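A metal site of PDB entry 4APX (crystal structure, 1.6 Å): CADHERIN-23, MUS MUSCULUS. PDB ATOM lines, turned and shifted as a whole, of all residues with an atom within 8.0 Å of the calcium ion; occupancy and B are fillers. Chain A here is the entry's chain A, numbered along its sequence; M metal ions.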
ATOM      1  N   VAL A   3       1.856  -0.213 -27.753  1.00  0.00           N
ATOM      2  CA  VAL A   3       0.498   0.262 -28.014  1.00  0.00           C
ATOM      3  C   VAL A   3      -0.354  -0.943 -28.415  1.00  0.00           C
ATOM      4  O   VAL A   3       0.145  -1.921 -28.970  1.00  0.00           O
ATOM      5  CB  VAL A   3       0.407   1.340 -29.138  1.00  0.00           C
ATOM      6  CG1 VAL A   3       1.249   2.562 -28.775  1.00  0.00           C
ATOM      7  CG2 VAL A   3       0.804   0.763 -30.501  1.00  0.00           C
ATOM      8  N   ASN A   4      -1.639  -0.877 -28.096  1.00  0.00           N
ATOM      9  CA  ASN A   4      -2.534  -1.964 -28.482  1.00  0.00           C
ATOM     10  C   ASN A   4      -2.559  -2.146 -29.987  1.00  0.00           C
ATOM     11  O   ASN A   4      -2.587  -1.152 -30.740  1.00  0.00           O
ATOM     12  CB  ASN A   4      -3.955  -1.682 -28.009  1.00  0.00           C
ATOM     13  CG  ASN A   4      -4.890  -2.836 -28.277  1.00  0.00           C
ATOM     14  OD1 ASN A   4      -4.598  -3.972 -27.918  1.00  0.00           O
ATOM     15  ND2 ASN A   4      -6.026  -2.550 -28.907  1.00  0.00           N
ATOM     16  N   ARG A   5      -2.538  -3.406 -30.411  1.00  0.00           N
ATOM     17  CA  ARG A   5      -2.789  -3.792 -31.802  1.00  0.00           C
ATOM     18  C   ARG A   5      -4.217  -4.305 -31.862  1.00  0.00           C
ATOM     19  O   ARG A   5      -4.600  -5.186 -31.087  1.00  0.00           O
ATOM     20  CB  ARG A   5      -1.861  -4.925 -32.253  1.00  0.00           C
ATOM     21  CG  ARG A   5      -0.472  -4.492 -32.704  1.00  0.00           C
ATOM     22  CD  ARG A   5       0.432  -4.116 -31.583  1.00  0.00           C
ATOM     23  NE  ARG A   5       0.710  -5.188 -30.626  1.00  0.00           N
ATOM     24  CZ  ARG A   5       1.669  -6.114 -30.741  1.00  0.00           C
ATOM     25  NH1 ARG A   5       2.469  -6.162 -31.811  1.00  0.00           N
ATOM     26  NH2 ARG A   5       1.819  -7.017 -29.780  1.00  0.00           N
ATOM     27  N   LEU A   6      -5.003  -3.760 -32.777  1.00  0.00           N
ATOM     28  CA  LEU A   6      -6.387  -4.186 -32.937  1.00  0.00           C
ATOM     29  C   LEU A   6      -6.452  -5.589 -33.561  1.00  0.00           C
ATOM     30  O   LEU A   6      -5.547  -5.999 -34.301  1.00  0.00           O
ATOM     31  CB  LEU A   6      -7.148  -3.163 -33.793  1.00  0.00           C
ATOM     32  CG  LEU A   6      -7.418  -1.802 -33.150  1.00  0.00           C
ATOM     33  CD1 LEU A   6      -7.916  -0.789 -34.168  1.00  0.00           C
ATOM     34  CD2 LEU A   6      -8.419  -1.960 -32.019  1.00  0.00           C
ATOM     35  N   PRO A   7      -7.519  -6.337 -33.246  1.00  0.00           N
ATOM     36  CA  PRO A   7      -7.673  -7.664 -33.855  1.00  0.00           C
ATOM     37  C   PRO A   7      -8.012  -7.601 -35.337  1.00  0.00           C
ATOM     38  O   PRO A   7      -8.369  -6.538 -35.848  1.00  0.00           O
ATOM     39  CB  PRO A   7      -8.819  -8.277 -33.039  1.00  0.00           C
ATOM     40  CG  PRO A   7      -9.648  -7.100 -32.618  1.00  0.00           C
ATOM     41  CD  PRO A   7      -8.633  -6.009 -32.337  1.00  0.00           C
ATOM     42  N   PHE A   8      -7.899  -8.737 -36.012  1.00  0.00           N
ATOM     43  CA  PHE A   8      -8.222  -8.852 -37.431  1.00  0.00           C
ATOM     44  C   PHE A   8      -8.863 -10.205 -37.726  1.00  0.00           C
ATOM     45  O   PHE A   8      -8.478 -11.236 -37.150  1.00  0.00           O
ATOM     46  CB  PHE A   8      -6.983  -8.604 -38.318  1.00  0.00           C
ATOM     47  CG  PHE A   8      -5.828  -9.517 -38.050  1.00  0.00           C
ATOM     48  CD1 PHE A   8      -4.861  -9.174 -37.110  1.00  0.00           C
ATOM     49  CD2 PHE A   8      -5.638 -10.687 -38.782  1.00  0.00           C
ATOM     50  CE1 PHE A   8      -3.769  -9.993 -36.860  1.00  0.00           C
ATOM     51  CE2 PHE A   8      -4.540 -11.520 -38.549  1.00  0.00           C
ATOM     52  CZ  PHE A   8      -3.599 -11.159 -37.583  1.00  0.00           C
ATOM     53  N   ARG A  36      -7.504 -13.001 -34.994  1.00  0.00           N
ATOM     54  CA  ARG A  36      -6.248 -13.017 -34.252  1.00  0.00           C
ATOM     55  C   ARG A  36      -5.960 -11.637 -33.676  1.00  0.00           C
ATOM     56  O   ARG A  36      -6.459 -10.615 -34.155  1.00  0.00           O
ATOM     57  CB  ARG A  36      -5.070 -13.428 -35.134  1.00  0.00           C
ATOM     58  CG  ARG A  36      -5.200 -14.727 -35.880  1.00  0.00           C
ATOM     59  CD  ARG A  36      -5.426 -15.925 -34.977  1.00  0.00           C
ATOM     60  NE  ARG A  36      -4.272 -16.312 -34.179  1.00  0.00           N
ATOM     61  CZ  ARG A  36      -4.318 -17.236 -33.220  1.00  0.00           C
ATOM     62  NH1 ARG A  36      -5.474 -17.856 -32.924  1.00  0.00           N
ATOM     63  NH2 ARG A  36      -3.234 -17.538 -32.533  1.00  0.00           N
ATOM     64  N   ASP A  37      -5.128 -11.607 -32.643  1.00  0.00           N
ATOM     65  CA  ASP A  37      -4.750 -10.350 -32.001  1.00  0.00           C
ATOM     66  C   ASP A  37      -3.300 -10.497 -31.605  1.00  0.00           C
ATOM     67  O   ASP A  37      -2.938 -11.461 -30.941  1.00  0.00           O
ATOM     68  CB  ASP A  37      -5.646 -10.120 -30.781  1.00  0.00           C
ATOM     69  CG  ASP A  37      -5.437  -8.769 -30.152  1.00  0.00           C
ATOM     70  OD1 ASP A  37      -4.380  -8.559 -29.499  1.00  0.00           O
ATOM     71  OD2 ASP A  37      -6.339  -7.919 -30.287  1.00  0.00           O
ATOM     72  N   MET A  38      -2.459  -9.553 -32.044  1.00  0.00           N
ATOM     73  CA  MET A  38      -1.028  -9.641 -31.771  1.00  0.00           C
ATOM     74  C   MET A  38      -0.656  -9.548 -30.303  1.00  0.00           C
ATOM     75  O   MET A  38       0.438  -9.991 -29.915  1.00  0.00           O
ATOM     76  CB  MET A  38      -0.230  -8.633 -32.594  1.00  0.00           C
ATOM     77  CG  MET A  38      -0.299  -8.883 -34.093  1.00  0.00           C
ATOM     78  SD  MET A  38       0.291 -10.527 -34.554  1.00  0.00           S
ATOM     79  CE  MET A  38      -1.224 -11.487 -34.582  1.00  0.00           C
ATOM     80  N   ASP A  39      -1.569  -9.009 -29.492  1.00  0.00           N
ATOM     81  CA  ASP A  39      -1.379  -8.945 -28.040  1.00  0.00           C
ATOM     82  C   ASP A  39      -1.894 -10.179 -27.297  1.00  0.00           C
ATOM     83  O   ASP A  39      -1.855 -10.211 -26.064  1.00  0.00           O
ATOM     84  CB  ASP A  39      -2.080  -7.702 -27.479  1.00  0.00           C
ATOM     85  CG  ASP A  39      -1.776  -6.459 -28.276  1.00  0.00           C
ATOM     86  OD1 ASP A  39      -0.604  -6.041 -28.316  1.00  0.00           O
ATOM     87  OD2 ASP A  39      -2.728  -5.896 -28.864  1.00  0.00           O
ATOM     88  N   ASN A  40      -2.396 -11.181 -28.037  1.00  0.00           N
ATOM     89  CA  ASN A  40      -3.019 -12.381 -27.501  1.00  0.00           C
ATOM     90  C   ASN A  40      -4.274 -12.049 -26.700  1.00  0.00           C
ATOM     91  O   ASN A  40      -4.667 -12.828 -25.836  1.00  0.00           O
ATOM     92  CB  ASN A  40      -2.079 -13.199 -26.586  1.00  0.00           C
ATOM     93  CG  ASN A  40      -0.784 -13.539 -27.249  1.00  0.00           C
ATOM     94  OD1 ASN A  40      -0.780 -14.126 -28.327  1.00  0.00           O
ATOM     95  ND2 ASN A  40       0.338 -13.210 -26.586  1.00  0.00           N
ATOM     96  N   ASP A  41      -4.905 -10.913 -27.011  1.00  0.00           N
ATOM     97  CA  ASP A  41      -6.103 -10.508 -26.286  1.00  0.00           C
ATOM     98  C   ASP A  41      -7.255 -11.469 -26.541  1.00  0.00           C
ATOM     99  O   ASP A  41      -7.414 -11.983 -27.642  1.00  0.00           O
ATOM    100  CB  ASP A  41      -6.537  -9.091 -26.685  1.00  0.00           C
ATOM    101  CG  ASP A  41      -5.574  -8.012 -26.227  1.00  0.00           C
ATOM    102  OD1 ASP A  41      -4.818  -8.216 -25.256  1.00  0.00           O
ATOM    103  OD2 ASP A  41      -5.574  -6.921 -26.849  1.00  0.00           O
ATOM    104  N   PRO A  42      -8.062 -11.717 -25.487  1.00  0.00           N
ATOM    105  CA  PRO A  42      -9.291 -12.468 -25.656  1.00  0.00           C
ATOM    106  C   PRO A  42     -10.275 -11.586 -26.423  1.00  0.00           C
ATOM    107  O   PRO A  42     -10.367 -10.378 -26.171  1.00  0.00           O
ATOM    108  CB  PRO A  42      -9.740 -12.741 -24.221  1.00  0.00           C
ATOM    109  CG  PRO A  42      -9.113 -11.750 -23.415  1.00  0.00           C
ATOM    110  CD  PRO A  42      -7.854 -11.285 -24.110  1.00  0.00           C
ATOM    111  N   LEU A  43     -10.963 -12.182 -27.382  1.00  0.00           N
ATOM    112  CA  LEU A  43     -11.796 -11.445 -28.309  1.00  0.00           C
ATOM    113  C   LEU A  43     -13.271 -11.709 -28.139  1.00  0.00           C
ATOM    114  O   LEU A  43     -13.696 -12.837 -27.822  1.00  0.00           O
ATOM    115  CB  LEU A  43     -11.375 -11.788 -29.736  1.00  0.00           C
ATOM    116  CG  LEU A  43      -9.897 -11.561 -30.001  1.00  0.00           C
ATOM    117  CD1 LEU A  43      -9.582 -11.940 -31.459  1.00  0.00           C
ATOM    118  CD2 LEU A  43      -9.503 -10.128 -29.736  1.00  0.00           C
ATOM    119  N   SER A  86     -13.806  -7.481 -31.114  1.00  0.00           N
ATOM    120  CA  SER A  86     -13.246  -6.514 -30.168  1.00  0.00           C
ATOM    121  C   SER A  86     -12.263  -7.149 -29.216  1.00  0.00           C
ATOM    122  O   SER A  86     -12.462  -8.290 -28.782  1.00  0.00           O
ATOM    123  CB  SER A  86     -14.382  -5.867 -29.367  1.00  0.00           C
ATOM    124  OG  SER A  86     -13.853  -5.083 -28.305  1.00  0.00           O
ATOM    125  N   ASP A  87     -11.194  -6.412 -28.897  1.00  0.00           N
ATOM    126  CA  ASP A  87     -10.226  -6.854 -27.910  1.00  0.00           C
ATOM    127  C   ASP A  87     -10.399  -6.065 -26.608  1.00  0.00           C
ATOM    128  O   ASP A  87      -9.475  -6.014 -25.798  1.00  0.00           O
ATOM    129  CB  ASP A  87      -8.787  -6.721 -28.411  1.00  0.00           C
ATOM    130  CG  ASP A  87      -8.386  -5.273 -28.651  1.00  0.00           C
ATOM    131  OD1 ASP A  87      -9.209  -4.363 -28.393  1.00  0.00           O
ATOM    132  OD2 ASP A  87      -7.241  -5.045 -29.098  1.00  0.00           O
ATOM    133  N   HIS A  88     -11.581  -5.457 -26.435  1.00  0.00           N
ATOM    134  CA  HIS A  88     -11.903  -4.658 -25.236  1.00  0.00           C
ATOM    135  C   HIS A  88     -11.280  -3.246 -25.251  1.00  0.00           C
ATOM    136  O   HIS A  88     -11.554  -2.446 -24.352  1.00  0.00           O
ATOM    137  CB  HIS A  88     -11.521  -5.382 -23.928  1.00  0.00           C
ATOM    138  CG  HIS A  88     -12.137  -6.746 -23.768  1.00  0.00           C
ATOM    139  ND1 HIS A  88     -11.433  -7.916 -23.972  1.00  0.00           N
ATOM    140  CD2 HIS A  88     -13.388  -7.125 -23.394  1.00  0.00           C
ATOM    141  CE1 HIS A  88     -12.221  -8.946 -23.748  1.00  0.00           C
ATOM    142  NE2 HIS A  88     -13.405  -8.496 -23.385  1.00  0.00           N
ATOM    143  N   GLN A  89     -10.420  -2.956 -26.222  1.00  0.00           N
ATOM    144  CA  GLN A  89      -9.879  -1.595 -26.389  1.00  0.00           C
ATOM    145  C   GLN A  89     -10.382  -0.931 -27.647  1.00  0.00           C
ATOM    146  O   GLN A  89     -10.496   0.290 -27.706  1.00  0.00           O
ATOM    147  CB  GLN A  89      -8.367  -1.609 -26.370  1.00  0.00           C
ATOM    148  CG  GLN A  89      -7.818  -1.946 -25.020  1.00  0.00           C
ATOM    149  CD  GLN A  89      -6.343  -1.685 -24.906  1.00  0.00           C
ATOM    150  OE1 GLN A  89      -5.905  -0.532 -24.930  1.00  0.00           O
ATOM    151  NE2 GLN A  89      -5.574  -2.755 -24.758  1.00  0.00           N
ATOM    152  N   GLY A  90     -10.658  -1.728 -28.659  1.00  0.00           N
ATOM    153  CA  GLY A  90     -11.224  -1.205 -29.892  1.00  0.00           C
ATOM    154  C   GLY A  90     -12.042  -2.293 -30.548  1.00  0.00           C
ATOM    155  O   GLY A  90     -11.937  -3.461 -30.191  1.00  0.00           O
HETATM  156 CA    CA M   1      -5.095  -6.130 -29.047  1.00  0.00          CA
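Six residues have an atom within 4 Å of the calcium ion: Asn 4, Arg 5, Asp 37, Asp 39, Asp 41 and Asp 87.
O of Arg 5 binds the calcium ion (2.3 Å).
OD2 of Asp 41 is bound to the calcium ion (2.4 Å).
The calcium ion is bound by OD2 of Asp 39 (2.4 Å).
OD2 of Asp 87 binds the calcium ion.
The calcium ion is bound by OD1 of Asn 4, at 2.5 Å.
The calcium ion is bound by OD2 of Asp 37 (2.5 Å).
OD1 of Asp 37 is bound to the calcium ion, 2.6 Å away.
The calcium ion has seven donor atoms within binding distance.
The backbone NH (N) of Gly 90 sits at hydrogen-bond distance from the side-chain carboxylate (OD1) of Asp 87.
The backbone NH (N) of Gln 89 sits at hydrogen-bond distance from the side-chain carboxylate (OD1) of Asp 87 (2.9 Å).
NH2 of Arg 5 lies within hydrogen-bond range of O of Met 38 (3.3 Å).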
